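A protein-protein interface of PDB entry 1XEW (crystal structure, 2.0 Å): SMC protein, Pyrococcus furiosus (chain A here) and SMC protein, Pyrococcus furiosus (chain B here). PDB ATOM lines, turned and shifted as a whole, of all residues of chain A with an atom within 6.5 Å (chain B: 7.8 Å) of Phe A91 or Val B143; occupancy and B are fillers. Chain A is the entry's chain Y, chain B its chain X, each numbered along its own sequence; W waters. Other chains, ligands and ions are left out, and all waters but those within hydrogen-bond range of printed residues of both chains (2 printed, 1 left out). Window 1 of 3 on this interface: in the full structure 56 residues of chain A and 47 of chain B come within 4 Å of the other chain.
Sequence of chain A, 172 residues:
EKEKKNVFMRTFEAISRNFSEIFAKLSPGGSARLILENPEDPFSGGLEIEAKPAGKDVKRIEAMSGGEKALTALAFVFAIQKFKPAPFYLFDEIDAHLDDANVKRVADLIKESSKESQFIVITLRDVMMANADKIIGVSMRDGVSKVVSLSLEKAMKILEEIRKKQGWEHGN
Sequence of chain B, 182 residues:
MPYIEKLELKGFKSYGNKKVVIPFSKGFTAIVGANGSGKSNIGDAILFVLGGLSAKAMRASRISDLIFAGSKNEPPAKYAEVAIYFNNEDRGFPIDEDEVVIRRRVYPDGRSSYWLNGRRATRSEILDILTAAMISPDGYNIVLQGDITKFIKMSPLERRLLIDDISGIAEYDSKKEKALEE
O of Phe A119 is in hydrogen-bond range of N of Thr B29 (3.1 Å). The backbone carbonyl oxygen of Thr B29 lies within hydrogen-bond range of the backbone NH of Val A121 (3.0 Å). The backbone NH of Ile B31 is in hydrogen-bond range of the backbone carbonyl oxygen of Val A121, 2.8 Å away. N of Thr A123 is in hydrogen-bond range of O of Ile B31 (3.1 Å). The backbone carbonyl oxygen (O) of Tyr B140 lies close to the side-chain amide oxygen (OE1) of Gln A81 (2.8 Å). The backbone carbonyl oxygen of Asn B141 lies within hydrogen-bond range of the backbone NH of Leu A90. The backbone NH of Val B143 sits at hydrogen-bond distance from the backbone carbonyl oxygen of Leu A90 (2.9 Å). O of Val B143 sits at hydrogen-bond distance from N of Asp A92 (2.9 Å).
The backbone NH (N) of Leu B144 is in hydrogen-bond range of the side-chain carboxylate (OD1) of Asp B147, 2.6 Å away. N of Ile A120 sits at hydrogen-bond distance from O of Tyr A89 (2.7 Å). O of Ile A120 is in hydrogen-bond range of N of Phe A91, 2.8 Å away. O of Phe A91 is in hydrogen-bond range of N of Ile A122, 2.7 Å away. The backbone NH (N) of Glu A93 is in hydrogen-bond range of the backbone carbonyl oxygen (O) of Ile A122, at 2.8 Å.
Among the printed residues, merely in contact across the chains: Val A77 with Phe B151 (3.2 Å), Tyr A89 with Asn B141 (3.3 Å), Phe A91 with Val B143 (3.5 Å), Gln A81 with Val B143 (3.5 Å), Asp A92 with Gln B145 (3.5 Å), Ile A122 with Ile B31 (3.5 Å), Val A121 with Phe B28 (3.6 Å), Ile A120 with Thr B29 (3.6 Å), Phe A119 with Phe B28 (3.6 Å), Glu A93 with Gln B145 (3.6 Å), Leu A90 with Ile B142 (3.7 Å), Ile A94 with Val B143 (3.7 Å), Ile A120 with Ile B31 (3.8 Å), Val A77 with Tyr B140 (3.9 Å), Gln A81 with Asn B141 (3.9 Å), Asp A92 with Leu B144 (3.9 Å), Phe A91 with Asn B141 (3.9 Å) and Val A77 with Val B143 (3.95 Å).
Of chain B, only Asn B141 (3.9 Å) and Val B143 (3.5 Å) come within 4 Å of Phe A91. Of chain A, only Val A77 (3.95 Å), Gln A81 (3.5 Å), Leu A90 (2.9 Å), Phe A91 (3.5 Å), Asp A92 (2.9 Å) and Ile A94 (3.7 Å) come within 4 Å of Val B143. Printed residues of chain A within 4 Å of Ile B142: Leu A90. Printed residues of chain B within 4 Å of Leu A90: Asn B141 (3.1 Å), Ile B142 (3.7 Å) and Val B143 (2.9 Å). Of the printed residues of chain A, Phe B28 touches Phe A119 and Val A121. Of the printed residues of chain B, Gln A81 touches Tyr B140, Asn B141 and Val B143. Phe A78 touches none of the printed residues of chain B.
Of the 15 printed residues of chain A, 13 touch a printed residue of chain B. Of the 16 printed residues of chain B, 10 touch a printed residue of chain A. Hydrophobic or aromatic side chains of chain B within 4 Å of the printed part of chain A: Phe B28, Ile B31, Val B143, Leu B144 and Phe B151. Among the printed residues, 26 pairs touch across the chains. Among the printed residues, no Asp or Glu carboxylate lies within 4 Å of a Lys or Arg side-chain nitrogen of the other chain.
Water W2 bridges OG1 of Thr B29 and O of Phe A119. Water W1 lies within hydrogen-bond range of the backbone carbonyl oxygen (O) of Ile B31 and the backbone carbonyl oxygen (O) of Thr A123.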
ATOM      1  N   VAL A  77     -12.399 -16.841  -0.398  1.00  0.00           N
ATOM      2  CA  VAL A  77     -12.704 -15.527  -0.920  1.00  0.00           C
ATOM      3  C   VAL A  77     -13.873 -14.895  -0.149  1.00  0.00           C
ATOM      4  O   VAL A  77     -13.807 -13.722   0.208  1.00  0.00           O
ATOM      5  CB  VAL A  77     -13.003 -15.512  -2.490  1.00  0.00           C
ATOM      6  CG1 VAL A  77     -12.750 -14.083  -3.072  1.00  0.00           C
ATOM      7  CG2 VAL A  77     -11.992 -16.403  -3.201  1.00  0.00           C
ATOM      8  N   PHE A  78     -14.942 -15.635   0.120  1.00  0.00           N
ATOM      9  CA  PHE A  78     -16.028 -15.068   0.926  1.00  0.00           C
ATOM     10  C   PHE A  78     -15.517 -14.558   2.323  1.00  0.00           C
ATOM     11  O   PHE A  78     -16.004 -13.531   2.834  1.00  0.00           O
ATOM     12  CB  PHE A  78     -17.105 -16.113   1.210  1.00  0.00           C
ATOM     13  CG  PHE A  78     -17.967 -16.468   0.002  1.00  0.00           C
ATOM     14  CD1 PHE A  78     -18.843 -17.564   0.063  1.00  0.00           C
ATOM     15  CD2 PHE A  78     -17.918 -15.730  -1.178  1.00  0.00           C
ATOM     16  CE1 PHE A  78     -19.663 -17.909  -1.016  1.00  0.00           C
ATOM     17  CE2 PHE A  78     -18.725 -16.072  -2.265  1.00  0.00           C
ATOM     18  CZ  PHE A  78     -19.589 -17.144  -2.190  1.00  0.00           C
ATOM     19  N   GLN A  81     -13.847 -11.219   1.794  1.00  0.00           N
ATOM     20  CA  GLN A  81     -14.899 -10.277   1.489  1.00  0.00           C
ATOM     21  C   GLN A  81     -15.666  -9.832   2.761  1.00  0.00           C
ATOM     22  O   GLN A  81     -15.976  -8.646   2.937  1.00  0.00           O
ATOM     23  CB  GLN A  81     -15.836 -10.915   0.439  1.00  0.00           C
ATOM     24  CG  GLN A  81     -15.225 -10.904  -1.053  1.00  0.00           C
ATOM     25  CD  GLN A  81     -16.060 -11.764  -1.976  1.00  0.00           C
ATOM     26  OE1 GLN A  81     -15.805 -11.923  -3.244  1.00  0.00           O
ATOM     27  NE2 GLN A  81     -17.061 -12.334  -1.399  1.00  0.00           N
ATOM     28  N   TYR A  89     -20.701  -6.940  -5.371  1.00  0.00           N
ATOM     29  CA  TYR A  89     -19.983  -8.152  -5.750  1.00  0.00           C
ATOM     30  C   TYR A  89     -20.421  -8.583  -7.151  1.00  0.00           C
ATOM     31  O   TYR A  89     -21.589  -8.436  -7.572  1.00  0.00           O
ATOM     32  CB  TYR A  89     -20.241  -9.299  -4.775  1.00  0.00           C
ATOM     33  CG  TYR A  89     -19.755  -8.924  -3.444  1.00  0.00           C
ATOM     34  CD1 TYR A  89     -20.586  -8.215  -2.587  1.00  0.00           C
ATOM     35  CD2 TYR A  89     -18.427  -9.130  -3.078  1.00  0.00           C
ATOM     36  CE1 TYR A  89     -20.124  -7.733  -1.418  1.00  0.00           C
ATOM     37  CE2 TYR A  89     -17.944  -8.622  -1.893  1.00  0.00           C
ATOM     38  CZ  TYR A  89     -18.807  -7.935  -1.075  1.00  0.00           C
ATOM     39  OH  TYR A  89     -18.416  -7.456   0.153  1.00  0.00           O
ATOM     40  N   LEU A  90     -19.436  -9.008  -7.908  1.00  0.00           N
ATOM     41  CA  LEU A  90     -19.717  -9.484  -9.236  1.00  0.00           C
ATOM     42  C   LEU A  90     -19.013 -10.858  -9.338  1.00  0.00           C
ATOM     43  O   LEU A  90     -17.779 -10.905  -9.339  1.00  0.00           O
ATOM     44  CB  LEU A  90     -19.047  -8.553 -10.241  1.00  0.00           C
ATOM     45  CG  LEU A  90     -19.115  -9.032 -11.714  1.00  0.00           C
ATOM     46  CD1 LEU A  90     -20.485  -8.915 -12.223  1.00  0.00           C
ATOM     47  CD2 LEU A  90     -18.166  -8.134 -12.541  1.00  0.00           C
ATOM     48  N   PHE A  91     -19.782 -11.929  -9.519  1.00  0.00           N
ATOM     49  CA  PHE A  91     -19.237 -13.268  -9.584  1.00  0.00           C
ATOM     50  C   PHE A  91     -19.548 -13.842 -10.933  1.00  0.00           C
ATOM     51  O   PHE A  91     -20.675 -13.903 -11.331  1.00  0.00           O
ATOM     52  CB  PHE A  91     -19.875 -14.164  -8.470  1.00  0.00           C
ATOM     53  CG  PHE A  91     -19.727 -13.610  -7.058  1.00  0.00           C
ATOM     54  CD1 PHE A  91     -20.567 -14.089  -6.034  1.00  0.00           C
ATOM     55  CD2 PHE A  91     -18.697 -12.722  -6.696  1.00  0.00           C
ATOM     56  CE1 PHE A  91     -20.406 -13.711  -4.660  1.00  0.00           C
ATOM     57  CE2 PHE A  91     -18.541 -12.336  -5.279  1.00  0.00           C
ATOM     58  CZ  PHE A  91     -19.410 -12.854  -4.309  1.00  0.00           C
ATOM     59  N   ASP A  92     -18.539 -14.356 -11.598  1.00  0.00           N
ATOM     60  CA  ASP A  92     -18.807 -14.849 -12.928  1.00  0.00           C
ATOM     61  C   ASP A  92     -18.631 -16.333 -12.920  1.00  0.00           C
ATOM     62  O   ASP A  92     -17.509 -16.805 -12.951  1.00  0.00           O
ATOM     63  CB  ASP A  92     -17.817 -14.205 -13.940  1.00  0.00           C
ATOM     64  CG  ASP A  92     -18.129 -14.568 -15.371  1.00  0.00           C
ATOM     65  OD1 ASP A  92     -17.560 -13.866 -16.258  1.00  0.00           O
ATOM     66  OD2 ASP A  92     -18.892 -15.570 -15.612  1.00  0.00           O
ATOM     67  N   GLU A  93     -19.736 -17.057 -12.887  1.00  0.00           N
ATOM     68  CA  GLU A  93     -19.663 -18.545 -12.914  1.00  0.00           C
ATOM     69  C   GLU A  93     -18.774 -19.193 -11.817  1.00  0.00           C
ATOM     70  O   GLU A  93     -18.049 -20.141 -12.054  1.00  0.00           O
ATOM     71  CB  GLU A  93     -19.206 -19.025 -14.319  1.00  0.00           C
ATOM     72  CG  GLU A  93     -20.262 -18.831 -15.463  1.00  0.00           C
ATOM     73  CD  GLU A  93     -21.460 -19.674 -15.306  1.00  0.00           C
ATOM     74  OE1 GLU A  93     -21.522 -20.583 -14.464  1.00  0.00           O
ATOM     75  OE2 GLU A  93     -22.409 -19.416 -16.044  1.00  0.00           O
ATOM     76  N   ILE A  94     -18.902 -18.676 -10.601  1.00  0.00           N
ATOM     77  CA  ILE A  94     -18.182 -19.222  -9.475  1.00  0.00           C
ATOM     78  C   ILE A  94     -18.777 -20.595  -9.053  1.00  0.00           C
ATOM     79  O   ILE A  94     -18.143 -21.328  -8.329  1.00  0.00           O
ATOM     80  CB  ILE A  94     -18.304 -18.252  -8.291  1.00  0.00           C
ATOM     81  CG1 ILE A  94     -19.785 -18.098  -7.953  1.00  0.00           C
ATOM     82  CG2 ILE A  94     -17.586 -16.951  -8.645  1.00  0.00           C
ATOM     83  CD1 ILE A  94     -20.057 -17.483  -6.589  1.00  0.00           C
ATOM     84  N   ILE A 110     -25.621 -16.148  -0.498  1.00  0.00           N
ATOM     85  CA  ILE A 110     -25.578 -14.951  -1.328  1.00  0.00           C
ATOM     86  C   ILE A 110     -26.870 -14.190  -1.146  1.00  0.00           C
ATOM     87  O   ILE A 110     -26.875 -12.963  -0.928  1.00  0.00           O
ATOM     88  CB  ILE A 110     -25.336 -15.336  -2.823  1.00  0.00           C
ATOM     89  CG1 ILE A 110     -23.863 -15.682  -3.011  1.00  0.00           C
ATOM     90  CG2 ILE A 110     -25.638 -14.129  -3.764  1.00  0.00           C
ATOM     91  CD1 ILE A 110     -23.597 -16.412  -4.422  1.00  0.00           C
ATOM     92  N   PHE A 119     -25.218  -7.968  -5.247  1.00  0.00           N
ATOM     93  CA  PHE A 119     -24.537  -9.134  -5.843  1.00  0.00           C
ATOM     94  C   PHE A 119     -25.009  -9.298  -7.249  1.00  0.00           C
ATOM     95  O   PHE A 119     -26.204  -9.243  -7.503  1.00  0.00           O
ATOM     96  CB  PHE A 119     -24.901 -10.418  -5.098  1.00  0.00           C
ATOM     97  CG  PHE A 119     -24.185 -10.572  -3.793  1.00  0.00           C
ATOM     98  CD1 PHE A 119     -24.633  -9.907  -2.681  1.00  0.00           C
ATOM     99  CD2 PHE A 119     -23.033 -11.378  -3.689  1.00  0.00           C
ATOM    100  CE1 PHE A 119     -23.940 -10.043  -1.451  1.00  0.00           C
ATOM    101  CE2 PHE A 119     -22.368 -11.507  -2.464  1.00  0.00           C
ATOM    102  CZ  PHE A 119     -22.850 -10.816  -1.353  1.00  0.00           C
ATOM    103  N   ILE A 120     -24.067  -9.473  -8.151  1.00  0.00           N
ATOM    104  CA  ILE A 120     -24.374  -9.675  -9.591  1.00  0.00           C
ATOM    105  C   ILE A 120     -23.662 -11.026  -9.854  1.00  0.00           C
ATOM    106  O   ILE A 120     -22.465 -11.216  -9.694  1.00  0.00           O
ATOM    107  CB  ILE A 120     -23.805  -8.487 -10.395  1.00  0.00           C
ATOM    108  CG1 ILE A 120     -24.521  -7.208  -9.962  1.00  0.00           C
ATOM    109  CG2 ILE A 120     -23.928  -8.731 -11.866  1.00  0.00           C
ATOM    110  CD1 ILE A 120     -23.727  -5.863 -10.473  1.00  0.00           C
ATOM    111  N   VAL A 121     -24.459 -11.996 -10.219  1.00  0.00           N
ATOM    112  CA  VAL A 121     -23.925 -13.320 -10.389  1.00  0.00           C
ATOM    113  C   VAL A 121     -24.207 -13.895 -11.734  1.00  0.00           C
ATOM    114  O   VAL A 121     -25.369 -14.053 -12.132  1.00  0.00           O
ATOM    115  CB  VAL A 121     -24.532 -14.304  -9.310  1.00  0.00           C
ATOM    116  CG1 VAL A 121     -23.803 -15.622  -9.468  1.00  0.00           C
ATOM    117  CG2 VAL A 121     -24.331 -13.754  -7.853  1.00  0.00           C
ATOM    118  N   ILE A 122     -23.160 -14.275 -12.419  1.00  0.00           N
ATOM    119  CA  ILE A 122     -23.411 -14.830 -13.722  1.00  0.00           C
ATOM    120  C   ILE A 122     -23.493 -16.325 -13.456  1.00  0.00           C
ATOM    121  O   ILE A 122     -22.516 -16.918 -12.996  1.00  0.00           O
ATOM    122  CB  ILE A 122     -22.263 -14.443 -14.653  1.00  0.00           C
ATOM    123  CG1 ILE A 122     -22.174 -12.889 -14.740  1.00  0.00           C
ATOM    124  CG2 ILE A 122     -22.478 -15.065 -16.034  1.00  0.00           C
ATOM    125  CD1 ILE A 122     -21.119 -12.359 -15.700  1.00  0.00           C
ATOM    126  N   THR A 123     -24.622 -16.947 -13.787  1.00  0.00           N
ATOM    127  CA  THR A 123     -24.809 -18.384 -13.488  1.00  0.00           C
ATOM    128  C   THR A 123     -25.746 -19.212 -14.491  1.00  0.00           C
ATOM    129  O   THR A 123     -26.532 -18.640 -15.228  1.00  0.00           O
ATOM    130  CB  THR A 123     -25.380 -18.469 -12.003  1.00  0.00           C
ATOM    131  OG1 THR A 123     -25.617 -19.816 -11.642  1.00  0.00           O
ATOM    132  CG2 THR A 123     -26.758 -17.743 -11.913  1.00  0.00           C
ATOM    133  N   PHE B  28     -29.971  -8.747  -5.383  1.00  0.00           N
ATOM    134  CA  PHE B  28     -29.413  -9.864  -6.105  1.00  0.00           C
ATOM    135  C   PHE B  28     -29.962  -9.952  -7.549  1.00  0.00           C
ATOM    136  O   PHE B  28     -31.154 -10.001  -7.770  1.00  0.00           O
ATOM    137  CB  PHE B  28     -29.770 -11.131  -5.272  1.00  0.00           C
ATOM    138  CG  PHE B  28     -29.203 -12.440  -5.813  1.00  0.00           C
ATOM    139  CD1 PHE B  28     -29.601 -13.642  -5.261  1.00  0.00           C
ATOM    140  CD2 PHE B  28     -28.313 -12.483  -6.883  1.00  0.00           C
ATOM    141  CE1 PHE B  28     -29.137 -14.854  -5.779  1.00  0.00           C
ATOM    142  CE2 PHE B  28     -27.851 -13.709  -7.388  1.00  0.00           C
ATOM    143  CZ  PHE B  28     -28.251 -14.877  -6.855  1.00  0.00           C
ATOM    144  N   THR B  29     -29.068  -9.949  -8.518  1.00  0.00           N
ATOM    145  CA  THR B  29     -29.398 -10.065  -9.953  1.00  0.00           C
ATOM    146  C   THR B  29     -28.648 -11.261 -10.465  1.00  0.00           C
ATOM    147  O   THR B  29     -27.426 -11.374 -10.230  1.00  0.00           O
ATOM    148  CB  THR B  29     -28.794  -8.868 -10.826  1.00  0.00           C
ATOM    149  OG1 THR B  29     -29.250  -7.633 -10.288  1.00  0.00           O
ATOM    150  CG2 THR B  29     -29.188  -8.948 -12.315  1.00  0.00           C
ATOM    151  N   ILE B  31     -27.436 -13.433 -13.989  1.00  0.00           N
ATOM    152  CA  ILE B  31     -27.220 -13.210 -15.428  1.00  0.00           C
ATOM    153  C   ILE B  31     -27.092 -14.553 -16.139  1.00  0.00           C
ATOM    154  O   ILE B  31     -26.100 -15.280 -15.982  1.00  0.00           O
ATOM    155  CB  ILE B  31     -25.915 -12.389 -15.703  1.00  0.00           C
ATOM    156  CG1 ILE B  31     -26.071 -11.005 -15.065  1.00  0.00           C
ATOM    157  CG2 ILE B  31     -25.700 -12.237 -17.217  1.00  0.00           C
ATOM    158  CD1 ILE B  31     -24.845 -10.128 -15.316  1.00  0.00           C
ATOM    159  N   LEU B  47     -14.355  -4.212 -15.576  1.00  0.00           N
ATOM    160  CA  LEU B  47     -12.936  -3.992 -15.306  1.00  0.00           C
ATOM    161  C   LEU B  47     -12.459  -2.775 -16.136  1.00  0.00           C
ATOM    162  O   LEU B  47     -11.668  -1.955 -15.641  1.00  0.00           O
ATOM    163  CB  LEU B  47     -12.057  -5.157 -15.757  1.00  0.00           C
ATOM    164  CG  LEU B  47     -12.247  -6.460 -14.948  1.00  0.00           C
ATOM    165  CD1 LEU B  47     -11.353  -7.558 -15.523  1.00  0.00           C
ATOM    166  CD2 LEU B  47     -11.938  -6.156 -13.452  1.00  0.00           C
ATOM    167  N   GLY B 139     -10.279  -5.236  -6.512  1.00  0.00           N
ATOM    168  CA  GLY B 139     -10.892  -5.707  -5.307  1.00  0.00           C
ATOM    169  C   GLY B 139     -11.242  -7.203  -5.364  1.00  0.00           C
ATOM    170  O   GLY B 139     -11.468  -7.867  -6.455  1.00  0.00           O
ATOM    171  N   TYR B 140     -11.261  -7.735  -4.141  1.00  0.00           N
ATOM    172  CA  TYR B 140     -11.668  -9.111  -3.864  1.00  0.00           C
ATOM    173  C   TYR B 140     -13.143  -9.346  -4.189  1.00  0.00           C
ATOM    174  O   TYR B 140     -13.617 -10.498  -4.274  1.00  0.00           O
ATOM    175  CB  TYR B 140     -11.463  -9.356  -2.369  1.00  0.00           C
ATOM    176  CG  TYR B 140     -10.008  -9.600  -2.078  1.00  0.00           C
ATOM    177  CD1 TYR B 140      -9.260  -8.680  -1.433  1.00  0.00           C
ATOM    178  CD2 TYR B 140      -9.399 -10.777  -2.519  1.00  0.00           C
ATOM    179  CE1 TYR B 140      -7.858  -8.898  -1.199  1.00  0.00           C
ATOM    180  CE2 TYR B 140      -8.054 -11.033  -2.311  1.00  0.00           C
ATOM    181  CZ  TYR B 140      -7.270 -10.079  -1.633  1.00  0.00           C
ATOM    182  OH  TYR B 140      -5.956 -10.399  -1.338  1.00  0.00           O
ATOM    183  N   ASN B 141     -13.890  -8.241  -4.284  1.00  0.00           N
ATOM    184  CA  ASN B 141     -15.336  -8.293  -4.554  1.00  0.00           C
ATOM    185  C   ASN B 141     -15.659  -8.630  -6.014  1.00  0.00           C
ATOM    186  O   ASN B 141     -16.814  -8.950  -6.344  1.00  0.00           O
ATOM    187  CB  ASN B 141     -15.987  -6.939  -4.184  1.00  0.00           C
ATOM    188  CG  ASN B 141     -15.460  -5.845  -5.024  1.00  0.00           C
ATOM    189  OD1 ASN B 141     -14.274  -5.705  -5.149  1.00  0.00           O
ATOM    190  ND2 ASN B 141     -16.337  -5.101  -5.653  1.00  0.00           N
ATOM    191  N   ILE B 142     -14.632  -8.670  -6.867  1.00  0.00           N
ATOM    192  CA  ILE B 142     -14.817  -9.029  -8.309  1.00  0.00           C
ATOM    193  C   ILE B 142     -14.153 -10.403  -8.482  1.00  0.00           C
ATOM    194  O   ILE B 142     -12.932 -10.574  -8.253  1.00  0.00           O
ATOM    195  CB  ILE B 142     -14.138  -7.944  -9.218  1.00  0.00           C
ATOM    196  CG1 ILE B 142     -14.910  -6.643  -9.031  1.00  0.00           C
ATOM    197  CG2 ILE B 142     -14.215  -8.334 -10.737  1.00  0.00           C
ATOM    198  CD1 ILE B 142     -14.439  -5.544  -9.991  1.00  0.00           C
ATOM    199  N   VAL B 143     -14.988 -11.411  -8.746  1.00  0.00           N
ATOM    200  CA  VAL B 143     -14.450 -12.754  -8.872  1.00  0.00           C
ATOM    201  C   VAL B 143     -14.817 -13.260 -10.283  1.00  0.00           C
ATOM    202  O   VAL B 143     -15.930 -13.702 -10.563  1.00  0.00           O
ATOM    203  CB  VAL B 143     -15.043 -13.668  -7.773  1.00  0.00           C
ATOM    204  CG1 VAL B 143     -14.480 -15.095  -7.949  1.00  0.00           C
ATOM    205  CG2 VAL B 143     -14.710 -13.069  -6.354  1.00  0.00           C
ATOM    206  N   LEU B 144     -13.873 -13.109 -11.191  1.00  0.00           N
ATOM    207  CA  LEU B 144     -14.137 -13.497 -12.560  1.00  0.00           C
ATOM    208  C   LEU B 144     -13.650 -14.899 -12.726  1.00  0.00           C
ATOM    209  O   LEU B 144     -13.156 -15.545 -11.792  1.00  0.00           O
ATOM    210  CB  LEU B 144     -13.411 -12.535 -13.537  1.00  0.00           C
ATOM    211  CG  LEU B 144     -13.931 -11.103 -13.350  1.00  0.00           C
ATOM    212  CD1 LEU B 144     -13.445 -10.109 -14.429  1.00  0.00           C
ATOM    213  CD2 LEU B 144     -15.439 -11.170 -13.346  1.00  0.00           C
ATOM    214  N   GLN B 145     -13.782 -15.378 -13.943  1.00  0.00           N
ATOM    215  CA  GLN B 145     -13.322 -16.729 -14.290  1.00  0.00           C
ATOM    216  C   GLN B 145     -11.784 -16.689 -14.189  1.00  0.00           C
ATOM    217  O   GLN B 145     -11.168 -15.779 -14.757  1.00  0.00           O
ATOM    218  CB  GLN B 145     -13.732 -16.910 -15.723  1.00  0.00           C
ATOM    219  CG  GLN B 145     -15.141 -16.608 -15.842  1.00  0.00           C
ATOM    220  CD  GLN B 145     -15.820 -17.888 -16.074  1.00  0.00           C
ATOM    221  OE1 GLN B 145     -15.733 -18.809 -15.231  1.00  0.00           O
ATOM    222  NE2 GLN B 145     -16.471 -18.011 -17.242  1.00  0.00           N
ATOM    223  N   GLY B 146     -11.143 -17.643 -13.536  1.00  0.00           N
ATOM    224  CA  GLY B 146      -9.702 -17.489 -13.441  1.00  0.00           C
ATOM    225  C   GLY B 146      -9.325 -17.070 -12.025  1.00  0.00           C
ATOM    226  O   GLY B 146      -8.178 -17.357 -11.579  1.00  0.00           O
ATOM    227  N   ASP B 147     -10.272 -16.406 -11.320  1.00  0.00           N
ATOM    228  CA  ASP B 147      -9.999 -15.941  -9.970  1.00  0.00           C
ATOM    229  C   ASP B 147     -10.085 -17.131  -8.997  1.00  0.00           C
ATOM    230  O   ASP B 147      -9.351 -17.174  -8.041  1.00  0.00           O
ATOM    231  CB  ASP B 147     -10.986 -14.867  -9.557  1.00  0.00           C
ATOM    232  CG  ASP B 147     -10.546 -13.530  -9.964  1.00  0.00           C
ATOM    233  OD1 ASP B 147     -11.392 -12.688 -10.375  1.00  0.00           O
ATOM    234  OD2 ASP B 147      -9.320 -13.322  -9.903  1.00  0.00           O
ATOM    235  N   ILE B 148     -11.007 -18.053  -9.243  1.00  0.00           N
ATOM    236  CA  ILE B 148     -11.125 -19.232  -8.403  1.00  0.00           C
ATOM    237  C   ILE B 148      -9.898 -20.155  -8.665  1.00  0.00           C
ATOM    238  O   ILE B 148      -9.312 -20.774  -7.739  1.00  0.00           O
ATOM    239  CB  ILE B 148     -12.482 -19.978  -8.630  1.00  0.00           C
ATOM    240  CG1 ILE B 148     -13.639 -19.162  -8.084  1.00  0.00           C
ATOM    241  CG2 ILE B 148     -12.459 -21.306  -7.931  1.00  0.00           C
ATOM    242  CD1 ILE B 148     -13.538 -18.788  -6.583  1.00  0.00           C
ATOM    243  N   THR B 149      -9.470 -20.283  -9.905  1.00  0.00           N
ATOM    244  CA  THR B 149      -8.264 -21.110 -10.102  1.00  0.00           C
ATOM    245  C   THR B 149      -7.065 -20.496  -9.329  1.00  0.00           C
ATOM    246  O   THR B 149      -6.226 -21.204  -8.780  1.00  0.00           O
ATOM    247  CB  THR B 149      -7.829 -21.179 -11.567  1.00  0.00           C
ATOM    248  OG1 THR B 149      -8.832 -21.837 -12.335  1.00  0.00           O
ATOM    249  CG2 THR B 149      -6.580 -21.998 -11.672  1.00  0.00           C
ATOM    250  N   PHE B 151      -7.026 -18.870  -6.539  1.00  0.00           N
ATOM    251  CA  PHE B 151      -7.152 -19.162  -5.088  1.00  0.00           C
ATOM    252  C   PHE B 151      -6.851 -20.595  -4.773  1.00  0.00           C
ATOM    253  O   PHE B 151      -6.186 -20.908  -3.780  1.00  0.00           O
ATOM    254  CB  PHE B 151      -8.540 -18.646  -4.572  1.00  0.00           C
ATOM    255  CG  PHE B 151      -8.578 -17.110  -4.417  1.00  0.00           C
ATOM    256  CD1 PHE B 151      -9.489 -16.346  -5.123  1.00  0.00           C
ATOM    257  CD2 PHE B 151      -7.616 -16.440  -3.628  1.00  0.00           C
ATOM    258  CE1 PHE B 151      -9.469 -14.910  -5.082  1.00  0.00           C
ATOM    259  CE2 PHE B 151      -7.572 -14.983  -3.567  1.00  0.00           C
ATOM    260  CZ  PHE B 151      -8.489 -14.246  -4.286  1.00  0.00           C
HETATM  261  O   HOH W   1     -24.959 -17.274 -17.274  1.00  0.00           O
HETATM  262  O   HOH W   2     -27.925  -6.873  -8.401  1.00  0.00           O
